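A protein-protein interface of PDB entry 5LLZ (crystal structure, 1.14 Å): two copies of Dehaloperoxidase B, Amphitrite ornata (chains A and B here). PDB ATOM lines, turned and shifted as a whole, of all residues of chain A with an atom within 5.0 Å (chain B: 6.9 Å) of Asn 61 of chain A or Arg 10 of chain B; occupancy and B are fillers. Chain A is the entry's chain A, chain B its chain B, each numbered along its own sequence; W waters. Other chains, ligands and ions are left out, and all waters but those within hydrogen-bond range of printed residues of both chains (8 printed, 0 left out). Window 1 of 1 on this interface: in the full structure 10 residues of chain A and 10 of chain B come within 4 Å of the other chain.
Arg 10 of chain A touches its own counterpart, Arg 10 of chain B.
Arg 10 of chain A touches Asn 61 of chain B, and with the chains exchanged Asn 61 of chain A touches Arg 10 of chain B.
Asn 61 of chain A touches Leu 13 of chain B, but with the chains exchanged Leu 13 of chain A does not touch Asn 61 of chain B (6.7 Å).
Asp 68 of chain A touches Arg 10 of chain B, but with the chains exchanged Arg 10 of chain A does not touch Asp 68 of chain B (5.5 Å).
Of the printed residues of chain B, Arg 10 of chain A touches Arg 10 (3.6 Å) and Asn 61 (3.4 Å).
Val 59 of chain A touches none of the printed residues of chain B.
Asn 61 of chain A touches three residues of chain B.
Of the printed residues of chain B, Asp 68 of chain A touches Arg 10 (3.96 Å).
Arg 10 of chain B touches just these residues of chain A: Arg 10, Asn 61 and Asp 68.
Printed residues of chain A within 4 Å of Gly 11 of chain B: Lys 58 (3.9 Å), Asn 61 (3.4 Å) and Glu 65 (3.9 Å).
Met 64 of chain B touches none of the printed residues of chain A.
The nearest printed residue of chain A that does not touch Gly 11 of chain B is Leu 62 of chain A (5.4 Å).
Printed residues of chain B that touch a printed residue of chain A: Ala 7, Arg 10, Gly 11, Asp 12, Leu 13, Arg 14, Glu 57 and Asn 61.
Among the printed residues, 12 pairs touch across the chains.
Among the printed residues, Asp or Glu carboxylates within 4 Å of a Lys or Arg side-chain nitrogen of the other chain: Asp 68 of chain A with Arg 10 of chain B.
NH1 of Arg 10 of chain A is in salt-bridge range of OD2 of Asp 68 of chain A, at 3.0 Å.
The guanidinium group (NH1) of Arg 10 of chain B lies within salt-bridge range of the side-chain carboxylate (OD2) of Asp 68 of chain B, 3.2 Å away.
The side-chain amide nitrogen of Asn 61 of chain A sits close to the backbone carbonyl oxygen of Glu 57 of chain A (3.4 Å).
The guanidinium group (NH1) of Arg 14 of chain B is in salt-bridge range of the side-chain carboxylate (OE1) of Glu 57 of chain B.
CZ of Arg 10 of chain B touches NH1 of Arg 10 of chain A (3.6 Å).
Arg 10 of chain A touches Asn 61 of chain B (CB to OD1, 3.4 Å).
CD of Arg 14 of chain B touches OE1 of Glu 57 of chain A (3.7 Å).
Gly 11 of chain B touches Lys 58 of chain A (O to CG, 3.9 Å).
OD1 of Asp 12 of chain B touches CE of Lys 58 of chain A (3.4 Å).
Leu 13 of chain B touches Asn 61 of chain A (N to ND2, 3.8 Å).
Glu 65 of chain A touches Ala 7 of chain B.
Glu 65 of chain A touches Gly 11 of chain B (OE2 to N, 3.9 Å).
Water W7 bridges OE2 of Glu 65 of chain A (2.4 Å) and O of Ala 7 of chain B (2.8 Å).
Water W3 bridges the backbone carbonyl oxygen of Gly 11 of chain B (2.8 Å) and the backbone carbonyl oxygen of Lys 58 of chain A (3.1 Å).
Water W1 bridges O of Arg 10 of chain B (2.8 Å) and OD1 of Asn 61 of chain A (2.9 Å).
Water W5 lies within hydrogen-bond range of the guanidinium group of Arg 10 of chain A (2.9 Å) and the side-chain carboxylate of Glu 65 of chain B (3.2 Å).
Water W2 lies within hydrogen-bond range of the side-chain carboxylate of Asp 68 of chain A (3.0 Å), the guanidinium group of Arg 10 of chain A (3.0 Å) and the guanidinium group of Arg 10 of chain B (3.2 Å).
Water W6 bridges OD1 of Asn 61 of chain B (3.3 Å) and NE of Arg 10 of chain A (3.4 Å).
O of Arg 10 of chain B sits close to ND2 of Asn 61 of chain A.
OD2 of Asp 68 of chain A is in salt-bridge range of NH1 of Arg 10 of chain B (3.96 Å).
ND2 of Asn 61 of chain A lies within hydrogen-bond range of O of Gly 11 of chain B, at 3.4 Å.
The side-chain carboxylate of Glu 57 of chain B sits close to the side-chain carboxylate of Glu 57 of chain A (2.7 Å).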
ATOM      1  N   ARG A  10       3.815   2.392  21.608  1.00  0.00           N
ATOM      2  CA  ARG A  10       3.286   3.528  20.843  1.00  0.00           C
ATOM      3  C   ARG A  10       4.276   3.966  19.732  1.00  0.00           C
ATOM      4  O   ARG A  10       3.806   4.418  18.656  1.00  0.00           O
ATOM      5  CB  ARG A  10       2.948   4.730  21.749  1.00  0.00           C
ATOM      6  CG  ARG A  10       1.631   4.624  22.465  1.00  0.00           C
ATOM      7  CD  ARG A  10       1.396   5.811  23.386  1.00  0.00           C
ATOM      8  NE  ARG A  10       0.019   5.882  23.847  1.00  0.00           N
ATOM      9  CZ  ARG A  10      -0.436   6.471  24.951  1.00  0.00           C
ATOM     10  NH1 ARG A  10       0.394   7.003  25.858  1.00  0.00           N
ATOM     11  NH2 ARG A  10      -1.770   6.495  25.185  1.00  0.00           N
ATOM     12  N   LEU A  13       3.406   1.376  16.830  1.00  0.00           N
ATOM     13  CA  LEU A  13       2.110   0.791  17.229  1.00  0.00           C
ATOM     14  C   LEU A  13       1.458  -0.090  16.187  1.00  0.00           C
ATOM     15  O   LEU A  13       0.878  -1.135  16.502  1.00  0.00           O
ATOM     16  CB  LEU A  13       1.103   1.855  17.766  1.00  0.00           C
ATOM     17  CG  LEU A  13      -0.026   1.297  18.678  1.00  0.00           C
ATOM     18  CD1 LEU A  13       0.496   0.424  19.856  1.00  0.00           C
ATOM     19  CD2 LEU A  13      -0.813   2.400  19.340  1.00  0.00           C
ATOM     20  N   GLU A  57      -5.779  -1.585  14.958  1.00  0.00           N
ATOM     21  CA  GLU A  57      -5.226  -0.266  15.310  1.00  0.00           C
ATOM     22  C   GLU A  57      -6.060   0.383  16.458  1.00  0.00           C
ATOM     23  O   GLU A  57      -5.507   0.883  17.454  1.00  0.00           O
ATOM     24  CB  GLU A  57      -5.309   0.698  14.119  1.00  0.00           C
ATOM     25  CG  GLU A  57      -4.386   1.874  14.334  1.00  0.00           C
ATOM     26  CD  GLU A  57      -2.988   1.695  13.748  1.00  0.00           C
ATOM     27  OE1 GLU A  57      -2.572   2.687  13.175  1.00  0.00           O
ATOM     28  OE2 GLU A  57      -2.320   0.604  13.828  1.00  0.00           O
ATOM     29  N   LYS A  58      -7.392   0.354  16.304  1.00  0.00           N
ATOM     30  CA  LYS A  58      -8.196   0.986  17.321  1.00  0.00           C
ATOM     31  C   LYS A  58      -8.160   0.214  18.660  1.00  0.00           C
ATOM     32  O   LYS A  58      -8.138   0.875  19.731  1.00  0.00           O
ATOM     33  CB  LYS A  58      -9.595   1.242  16.717  1.00  0.00           C
ATOM     34  CG  LYS A  58      -9.490   2.435  15.729  1.00  0.00           C
ATOM     35  CD  LYS A  58     -10.620   2.524  14.744  1.00  0.00           C
ATOM     36  CE  LYS A  58     -10.636   3.818  13.958  1.00  0.00           C
ATOM     37  NZ  LYS A  58     -11.796   3.722  12.999  1.00  0.00           N
ATOM     38  N   VAL A  59      -8.042  -1.133  18.654  1.00  0.00           N
ATOM     39  CA  VAL A  59      -7.846  -1.966  19.891  1.00  0.00           C
ATOM     40  C   VAL A  59      -6.648  -1.385  20.607  1.00  0.00           C
ATOM     41  O   VAL A  59      -6.721  -1.106  21.827  1.00  0.00           O
ATOM     42  CB  VAL A  59      -7.566  -3.507  19.630  1.00  0.00           C
ATOM     43  CG1 VAL A  59      -6.950  -4.230  20.852  1.00  0.00           C
ATOM     44  CG2 VAL A  59      -8.780  -4.271  19.158  1.00  0.00           C
ATOM     45  N   PHE A  60      -5.516  -1.286  19.927  1.00  0.00           N
ATOM     46  CA  PHE A  60      -4.282  -0.923  20.589  1.00  0.00           C
ATOM     47  C   PHE A  60      -4.201   0.578  20.942  1.00  0.00           C
ATOM     48  O   PHE A  60      -3.653   0.929  22.000  1.00  0.00           O
ATOM     49  CB  PHE A  60      -3.040  -1.466  19.848  1.00  0.00           C
ATOM     50  CG  PHE A  60      -2.808  -2.923  20.148  1.00  0.00           C
ATOM     51  CD1 PHE A  60      -3.590  -3.938  19.545  1.00  0.00           C
ATOM     52  CD2 PHE A  60      -1.899  -3.292  21.138  1.00  0.00           C
ATOM     53  CE1 PHE A  60      -3.380  -5.283  19.901  1.00  0.00           C
ATOM     54  CE2 PHE A  60      -1.688  -4.638  21.472  1.00  0.00           C
ATOM     55  CZ  PHE A  60      -2.458  -5.610  20.875  1.00  0.00           C
ATOM     56  N   ASN A  61      -4.755   1.462  20.091  1.00  0.00           N
ATOM     57  CA  ASN A  61      -4.808   2.880  20.481  1.00  0.00           C
ATOM     58  C   ASN A  61      -5.520   3.036  21.814  1.00  0.00           C
ATOM     59  O   ASN A  61      -5.013   3.738  22.743  1.00  0.00           O
ATOM     60  CB  ASN A  61      -5.539   3.743  19.417  1.00  0.00           C
ATOM     61  CG  ASN A  61      -4.754   3.973  18.144  1.00  0.00           C
ATOM     62  OD1 ASN A  61      -3.531   3.919  18.130  1.00  0.00           O
ATOM     63  ND2 ASN A  61      -5.475   4.294  17.044  1.00  0.00           N
ATOM     64  N   LEU A  62      -6.704   2.427  21.934  1.00  0.00           N
ATOM     65  CA  LEU A  62      -7.475   2.527  23.175  1.00  0.00           C
ATOM     66  C   LEU A  62      -6.848   1.784  24.335  1.00  0.00           C
ATOM     67  O   LEU A  62      -6.820   2.279  25.485  1.00  0.00           O
ATOM     68  CB  LEU A  62      -8.948   2.152  22.997  1.00  0.00           C
ATOM     69  CG  LEU A  62      -9.887   2.349  24.210  1.00  0.00           C
ATOM     70  CD1 LEU A  62      -9.830   3.775  24.850  1.00  0.00           C
ATOM     71  CD2 LEU A  62     -11.311   1.947  23.840  1.00  0.00           C
ATOM     72  N   MET A  63      -6.306   0.575  24.080  1.00  0.00           N
ATOM     73  CA  MET A  63      -5.652  -0.177  25.169  1.00  0.00           C
ATOM     74  C   MET A  63      -4.490   0.620  25.775  1.00  0.00           C
ATOM     75  O   MET A  63      -4.341   0.577  27.012  1.00  0.00           O
ATOM     76  CB  MET A  63      -5.092  -1.544  24.661  1.00  0.00           C
ATOM     77  CG  MET A  63      -4.563  -2.438  25.770  1.00  0.00           C
ATOM     78  SD  MET A  63      -3.441  -3.784  25.204  1.00  0.00           S
ATOM     79  CE  MET A  63      -4.571  -4.791  24.234  1.00  0.00           C
ATOM     80  N   MET A  64      -3.704   1.278  24.942  1.00  0.00           N
ATOM     81  CA  MET A  64      -2.621   2.115  25.486  1.00  0.00           C
ATOM     82  C   MET A  64      -3.113   3.262  26.362  1.00  0.00           C
ATOM     83  O   MET A  64      -2.456   3.617  27.357  1.00  0.00           O
ATOM     84  CB  MET A  64      -1.649   2.599  24.398  1.00  0.00           C
ATOM     85  CG  MET A  64      -0.887   1.512  23.680  1.00  0.00           C
ATOM     86  SD  MET A  64       0.143   0.418  24.730  1.00  0.00           S
ATOM     87  CE  MET A  64      -0.929  -1.007  24.961  1.00  0.00           C
ATOM     88  N   GLU A  65      -4.244   3.879  25.996  1.00  0.00           N
ATOM     89  CA  GLU A  65      -4.844   4.913  26.864  1.00  0.00           C
ATOM     90  C   GLU A  65      -5.325   4.348  28.193  1.00  0.00           C
ATOM     91  O   GLU A  65      -5.159   4.998  29.249  1.00  0.00           O
ATOM     92  CB  GLU A  65      -5.974   5.644  26.133  1.00  0.00           C
ATOM     93  CG  GLU A  65      -5.538   6.418  24.896  1.00  0.00           C
ATOM     94  CD  GLU A  65      -6.710   7.097  24.313  1.00  0.00           C
ATOM     95  OE1 GLU A  65      -7.200   8.071  24.883  1.00  0.00           O
ATOM     96  OE2 GLU A  65      -7.229   6.510  23.375  1.00  0.00           O
ATOM     97  N   ASP A  68      -2.311   3.817  30.266  1.00  0.00           N
ATOM     98  CA  ASP A  68      -1.742   5.099  30.702  1.00  0.00           C
ATOM     99  C   ASP A  68      -2.543   5.723  31.855  1.00  0.00           C
ATOM    100  O   ASP A  68      -1.971   6.341  32.758  1.00  0.00           O
ATOM    101  CB  ASP A  68      -1.621   5.995  29.453  1.00  0.00           C
ATOM    102  CG  ASP A  68      -0.545   7.006  29.504  1.00  0.00           C
ATOM    103  OD1 ASP A  68       0.279   7.010  30.451  1.00  0.00           O
ATOM    104  OD2 ASP A  68      -0.540   7.856  28.567  1.00  0.00           O
ATOM    105  N   GLN B   4      -8.677  16.111  27.001  1.00  0.00           N
ATOM    106  CA  GLN B   4      -9.594  15.277  26.218  1.00  0.00           C
ATOM    107  C   GLN B   4      -9.220  15.268  24.746  1.00  0.00           C
ATOM    108  O   GLN B   4      -9.317  14.198  24.090  1.00  0.00           O
ATOM    109  CB  GLN B   4     -11.062  15.692  26.387  1.00  0.00           C
ATOM    110  CG  GLN B   4     -12.059  14.929  25.505  1.00  0.00           C
ATOM    111  CD  GLN B   4     -11.929  13.413  25.581  1.00  0.00           C
ATOM    112  OE1 GLN B   4     -11.732  12.878  26.682  1.00  0.00           O
ATOM    113  NE2 GLN B   4     -12.075  12.697  24.456  1.00  0.00           N
ATOM    114  N   ASP B   5      -8.787  16.385  24.175  1.00  0.00           N
ATOM    115  CA  ASP B   5      -8.426  16.418  22.751  1.00  0.00           C
ATOM    116  C   ASP B   5      -7.261  15.424  22.461  1.00  0.00           C
ATOM    117  O   ASP B   5      -7.251  14.793  21.412  1.00  0.00           O
ATOM    118  CB  ASP B   5      -7.998  17.806  22.335  1.00  0.00           C
ATOM    119  CG  ASP B   5      -9.147  18.848  22.344  1.00  0.00           C
ATOM    120  OD1 ASP B   5     -10.334  18.435  22.397  1.00  0.00           O
ATOM    121  OD2 ASP B   5      -8.812  20.047  22.281  1.00  0.00           O
ATOM    122  N   ILE B   6      -6.286  15.316  23.396  1.00  0.00           N
ATOM    123  CA  ILE B   6      -5.219  14.315  23.216  1.00  0.00           C
ATOM    124  C   ILE B   6      -5.816  12.900  23.108  1.00  0.00           C
ATOM    125  O   ILE B   6      -5.411  12.091  22.262  1.00  0.00           O
ATOM    126  CB  ILE B   6      -4.165  14.414  24.361  1.00  0.00           C
ATOM    127  CG1 ILE B   6      -3.485  15.791  24.371  1.00  0.00           C
ATOM    128  CG2 ILE B   6      -3.175  13.268  24.270  1.00  0.00           C
ATOM    129  CD1 ILE B   6      -2.673  16.039  25.628  1.00  0.00           C
ATOM    130  N   ALA B   7      -6.825  12.593  23.953  1.00  0.00           N
ATOM    131  CA  ALA B   7      -7.522  11.308  23.885  1.00  0.00           C
ATOM    132  C   ALA B   7      -8.303  11.134  22.586  1.00  0.00           C
ATOM    133  O   ALA B   7      -8.304  10.035  21.972  1.00  0.00           O
ATOM    134  CB  ALA B   7      -8.469  11.097  25.095  1.00  0.00           C
ATOM    135  N   THR B   8      -9.016  12.185  22.129  1.00  0.00           N
ATOM    136  CA  THR B   8      -9.712  12.127  20.843  1.00  0.00           C
ATOM    137  C   THR B   8      -8.732  11.801  19.679  1.00  0.00           C
ATOM    138  O   THR B   8      -8.974  10.866  18.896  1.00  0.00           O
ATOM    139  CB  THR B   8     -10.442  13.443  20.516  1.00  0.00           C
ATOM    140  OG1 THR B   8     -11.433  13.676  21.530  1.00  0.00           O
ATOM    141  CG2 THR B   8     -11.059  13.447  19.137  1.00  0.00           C
ATOM    142  N   LEU B   9      -7.628  12.510  19.612  1.00  0.00           N
ATOM    143  CA  LEU B   9      -6.653  12.330  18.540  1.00  0.00           C
ATOM    144  C   LEU B   9      -6.011  10.926  18.649  1.00  0.00           C
ATOM    145  O   LEU B   9      -5.945  10.172  17.658  1.00  0.00           O
ATOM    146  CB  LEU B   9      -5.574  13.423  18.588  1.00  0.00           C
ATOM    147  CG  LEU B   9      -6.115  14.837  18.255  1.00  0.00           C
ATOM    148  CD1 LEU B   9      -5.048  15.917  18.576  1.00  0.00           C
ATOM    149  CD2 LEU B   9      -6.597  15.014  16.823  1.00  0.00           C
ATOM    150  N   ARG B  10      -5.606  10.506  19.860  1.00  0.00           N
ATOM    151  CA  ARG B  10      -5.001   9.187  20.040  1.00  0.00           C
ATOM    152  C   ARG B  10      -5.938   8.057  19.642  1.00  0.00           C
ATOM    153  O   ARG B  10      -5.464   7.005  19.180  1.00  0.00           O
ATOM    154  CB  ARG B  10      -4.461   8.985  21.500  1.00  0.00           C
ATOM    155  CG  ARG B  10      -3.145   9.674  21.733  1.00  0.00           C
ATOM    156  CD  ARG B  10      -2.616   9.366  23.124  1.00  0.00           C
ATOM    157  NE  ARG B  10      -1.226   9.721  23.284  1.00  0.00           N
ATOM    158  CZ  ARG B  10      -0.672  10.111  24.455  1.00  0.00           C
ATOM    159  NH1 ARG B  10      -1.428  10.313  25.589  1.00  0.00           N
ATOM    160  NH2 ARG B  10       0.639  10.383  24.514  1.00  0.00           N
ATOM    161  N   GLY B  11      -7.243   8.198  19.907  1.00  0.00           N
ATOM    162  CA  GLY B  11      -8.161   7.128  19.618  1.00  0.00           C
ATOM    163  C   GLY B  11      -8.195   6.743  18.144  1.00  0.00           C
ATOM    164  O   GLY B  11      -8.478   5.563  17.830  1.00  0.00           O
ATOM    165  N   ASP B  12      -7.901   7.682  17.245  1.00  0.00           N
ATOM    166  CA  ASP B  12      -7.866   7.422  15.784  1.00  0.00           C
ATOM    167  C   ASP B  12      -6.642   8.119  15.159  1.00  0.00           C
ATOM    168  O   ASP B  12      -6.753   8.897  14.188  1.00  0.00           O
ATOM    169  CB  ASP B  12      -9.189   7.904  15.108  1.00  0.00           C
ATOM    170  CG  ASP B  12      -9.425   7.353  13.749  1.00  0.00           C
ATOM    171  OD1 ASP B  12      -8.664   6.449  13.310  1.00  0.00           O
ATOM    172  OD2 ASP B  12     -10.382   7.875  13.069  1.00  0.00           O
ATOM    173  N   LEU B  13      -5.464   7.838  15.744  1.00  0.00           N
ATOM    174  CA  LEU B  13      -4.277   8.667  15.483  1.00  0.00           C
ATOM    175  C   LEU B  13      -3.838   8.650  14.013  1.00  0.00           C
ATOM    176  O   LEU B  13      -3.464   9.711  13.492  1.00  0.00           O
ATOM    177  CB  LEU B  13      -3.137   8.280  16.414  1.00  0.00           C
ATOM    178  CG  LEU B  13      -1.987   9.263  16.491  1.00  0.00           C
ATOM    179  CD1 LEU B  13      -2.419  10.642  16.981  1.00  0.00           C
ATOM    180  CD2 LEU B  13      -0.826   8.743  17.358  1.00  0.00           C
ATOM    181  N   ARG B  14      -3.815   7.478  13.362  1.00  0.00           N
ATOM    182  CA  ARG B  14      -3.323   7.404  11.978  1.00  0.00           C
ATOM    183  C   ARG B  14      -4.179   8.268  11.041  1.00  0.00           C
ATOM    184  O   ARG B  14      -3.662   8.890  10.117  1.00  0.00           O
ATOM    185  CB  ARG B  14      -3.232   5.941  11.513  1.00  0.00           C
ATOM    186  CG  ARG B  14      -2.529   5.686  10.141  1.00  0.00           C
ATOM    187  CD  ARG B  14      -2.536   4.173   9.791  1.00  0.00           C
ATOM    188  NE  ARG B  14      -1.924   3.827   8.494  1.00  0.00           N
ATOM    189  CZ  ARG B  14      -0.629   3.594   8.289  1.00  0.00           C
ATOM    190  NH1 ARG B  14       0.231   3.548   9.271  1.00  0.00           N
ATOM    191  NH2 ARG B  14      -0.216   3.321   7.048  1.00  0.00           N
ATOM    192  N   TYR B  16      -6.283  10.962  11.887  1.00  0.00           N
ATOM    193  CA  TYR B  16      -6.103  12.384  12.199  1.00  0.00           C
ATOM    194  C   TYR B  16      -4.722  12.901  11.726  1.00  0.00           C
ATOM    195  O   TYR B  16      -4.640  14.031  11.243  1.00  0.00           O
ATOM    196  CB  TYR B  16      -6.273  12.684  13.712  1.00  0.00           C
ATOM    197  CG  TYR B  16      -7.711  12.753  14.195  1.00  0.00           C
ATOM    198  CD1 TYR B  16      -8.550  13.790  13.747  1.00  0.00           C
ATOM    199  CD2 TYR B  16      -8.231  11.866  15.113  1.00  0.00           C
ATOM    200  CE1 TYR B  16      -9.873  13.862  14.198  1.00  0.00           C
ATOM    201  CE2 TYR B  16      -9.544  11.954  15.567  1.00  0.00           C
ATOM    202  CZ  TYR B  16     -10.374  12.984  15.139  1.00  0.00           C
ATOM    203  OH  TYR B  16     -11.678  13.050  15.610  1.00  0.00           O
ATOM    204  N   GLU B  57       1.898   8.893  11.369  1.00  0.00           N
ATOM    205  CA  GLU B  57       1.464   8.325  12.672  1.00  0.00           C
ATOM    206  C   GLU B  57       2.582   8.466  13.729  1.00  0.00           C
ATOM    207  O   GLU B  57       2.325   8.853  14.847  1.00  0.00           O
ATOM    208  CB  GLU B  57       1.005   6.857  12.500  1.00  0.00           C
ATOM    209  CG  GLU B  57       0.391   6.105  13.695  1.00  0.00           C
ATOM    210  CD  GLU B  57      -0.058   4.620  13.350  1.00  0.00           C
ATOM    211  OE1 GLU B  57       0.040   4.043  12.190  1.00  0.00           O
ATOM    212  OE2 GLU B  57      -0.528   3.996  14.322  1.00  0.00           O
ATOM    213  N   PHE B  60       2.891  12.145  14.836  1.00  0.00           N
ATOM    214  CA  PHE B  60       1.822  12.559  15.760  1.00  0.00           C
ATOM    215  C   PHE B  60       1.854  11.819  17.093  1.00  0.00           C
ATOM    216  O   PHE B  60       1.434  12.393  18.129  1.00  0.00           O
ATOM    217  CB  PHE B  60       0.439  12.517  15.072  1.00  0.00           C
ATOM    218  CG  PHE B  60       0.182  13.752  14.249  1.00  0.00           C
ATOM    219  CD1 PHE B  60       0.846  13.992  13.025  1.00  0.00           C
ATOM    220  CD2 PHE B  60      -0.731  14.729  14.683  1.00  0.00           C
ATOM    221  CE1 PHE B  60       0.621  15.162  12.313  1.00  0.00           C
ATOM    222  CE2 PHE B  60      -0.969  15.882  13.952  1.00  0.00           C
ATOM    223  CZ  PHE B  60      -0.296  16.104  12.771  1.00  0.00           C
ATOM    224  N   ASN B  61       2.415  10.603  17.148  1.00  0.00           N
ATOM    225  CA  ASN B  61       2.661   9.967  18.442  1.00  0.00           C
ATOM    226  C   ASN B  61       3.595  10.851  19.281  1.00  0.00           C
ATOM    227  O   ASN B  61       3.338  11.088  20.482  1.00  0.00           O
ATOM    228  CB  ASN B  61       3.246   8.560  18.297  1.00  0.00           C
ATOM    229  CG  ASN B  61       3.693   8.012  19.597  1.00  0.00           C
ATOM    230  OD1 ASN B  61       2.884   7.907  20.543  1.00  0.00           O
ATOM    231  ND2 ASN B  61       4.977   7.669  19.689  1.00  0.00           N
ATOM    232  N   LEU B  62       4.729  11.271  18.716  1.00  0.00           N
ATOM    233  CA  LEU B  62       5.644  12.181  19.472  1.00  0.00           C
ATOM    234  C   LEU B  62       4.946  13.509  19.818  1.00  0.00           C
ATOM    235  O   LEU B  62       5.079  13.997  20.988  1.00  0.00           O
ATOM    236  CB  LEU B  62       6.968  12.397  18.729  1.00  0.00           C
ATOM    237  CG  LEU B  62       7.990  13.291  19.472  1.00  0.00           C
ATOM    238  CD1 LEU B  62       8.334  12.775  20.848  1.00  0.00           C
ATOM    239  CD2 LEU B  62       9.207  13.447  18.576  1.00  0.00           C
ATOM    240  N   MET B  63       4.184  14.064  18.906  1.00  0.00           N
ATOM    241  CA  MET B  63       3.478  15.323  19.215  1.00  0.00           C
ATOM    242  C   MET B  63       2.561  15.130  20.452  1.00  0.00           C
ATOM    243  O   MET B  63       2.458  16.021  21.310  1.00  0.00           O
ATOM    244  CB  MET B  63       2.627  15.828  18.003  1.00  0.00           C
ATOM    245  CG  MET B  63       2.123  17.246  18.230  1.00  0.00           C
ATOM    246  SD  MET B  63       0.888  17.773  16.988  1.00  0.00           S
ATOM    247  CE  MET B  63       1.869  17.826  15.491  1.00  0.00           C
ATOM    248  N   MET B  64       1.811  14.031  20.486  1.00  0.00           N
ATOM    249  CA  MET B  64       0.885  13.778  21.612  1.00  0.00           C
ATOM    250  C   MET B  64       1.654  13.558  22.923  1.00  0.00           C
ATOM    251  O   MET B  64       1.148  13.923  24.003  1.00  0.00           O
ATOM    252  CB  MET B  64      -0.099  12.623  21.333  1.00  0.00           C
ATOM    253  CG  MET B  64      -1.072  12.862  20.183  1.00  0.00           C
ATOM    254  SD  MET B  64      -2.105  14.366  20.365  1.00  0.00           S
ATOM    255  CE  MET B  64      -1.188  15.574  19.354  1.00  0.00           C
ATOM    256  N   GLU B  65       2.830  12.894  22.877  1.00  0.00           N
ATOM    257  CA  GLU B  65       3.654  12.757  24.108  1.00  0.00           C
ATOM    258  C   GLU B  65       4.081  14.128  24.656  1.00  0.00           C
ATOM    259  O   GLU B  65       4.009  14.373  25.882  1.00  0.00           O
ATOM    260  CB  GLU B  65       4.886  11.855  23.833  1.00  0.00           C
ATOM    261  CG  GLU B  65       4.507  10.393  23.644  1.00  0.00           C
ATOM    262  CD  GLU B  65       5.510   9.419  23.212  1.00  0.00           C
ATOM    263  OE1 GLU B  65       5.334   8.194  23.574  1.00  0.00           O
ATOM    264  OE2 GLU B  65       6.459   9.837  22.544  1.00  0.00           O
ATOM    265  N   VAL B  66       4.548  15.005  23.743  1.00  0.00           N
ATOM    266  CA  VAL B  66       4.929  16.379  24.131  1.00  0.00           C
ATOM    267  C   VAL B  66       3.741  17.111  24.719  1.00  0.00           C
ATOM    268  O   VAL B  66       3.840  17.809  25.745  1.00  0.00           O
ATOM    269  CB  VAL B  66       5.613  17.089  22.964  1.00  0.00           C
ATOM    270  CG1 VAL B  66       5.943  18.537  23.315  1.00  0.00           C
ATOM    271  CG2 VAL B  66       6.907  16.356  22.552  1.00  0.00           C
ATOM    272  N   ASP B  68       1.008  15.853  26.115  1.00  0.00           N
ATOM    273  CA  ASP B  68       0.589  15.280  27.389  1.00  0.00           C
ATOM    274  C   ASP B  68       1.526  15.666  28.543  1.00  0.00           C
ATOM    275  O   ASP B  68       1.079  15.762  29.695  1.00  0.00           O
ATOM    276  CB  ASP B  68       0.447  13.767  27.272  1.00  0.00           C
ATOM    277  CG  ASP B  68      -0.564  13.160  28.201  1.00  0.00           C
ATOM    278  OD1 ASP B  68      -1.435  13.833  28.785  1.00  0.00           O
ATOM    279  OD2 ASP B  68      -0.538  11.888  28.192  1.00  0.00           O
HETATM  280  O   HOH W   1      -2.821   6.183  19.749  1.00  0.00           O
HETATM  281  O   HOH W   2      -3.172   8.158  27.230  1.00  0.00           O
HETATM  282  O   HOH W   3      -9.510   3.644  19.608  1.00  0.00           O
HETATM  283  O   HOH W   4      -4.781  10.067  25.933  1.00  0.00           O
HETATM  284  O   HOH W   5       3.302   7.182  25.888  1.00  0.00           O
HETATM  285  O   HOH W   6      -0.191   6.752  20.560  1.00  0.00           O
HETATM  286  O   HOH W   7      -9.336   7.629  22.890  1.00  0.00           O
HETATM  287  O   HOH W   8      -0.989   5.014  16.769  1.00  0.00           O
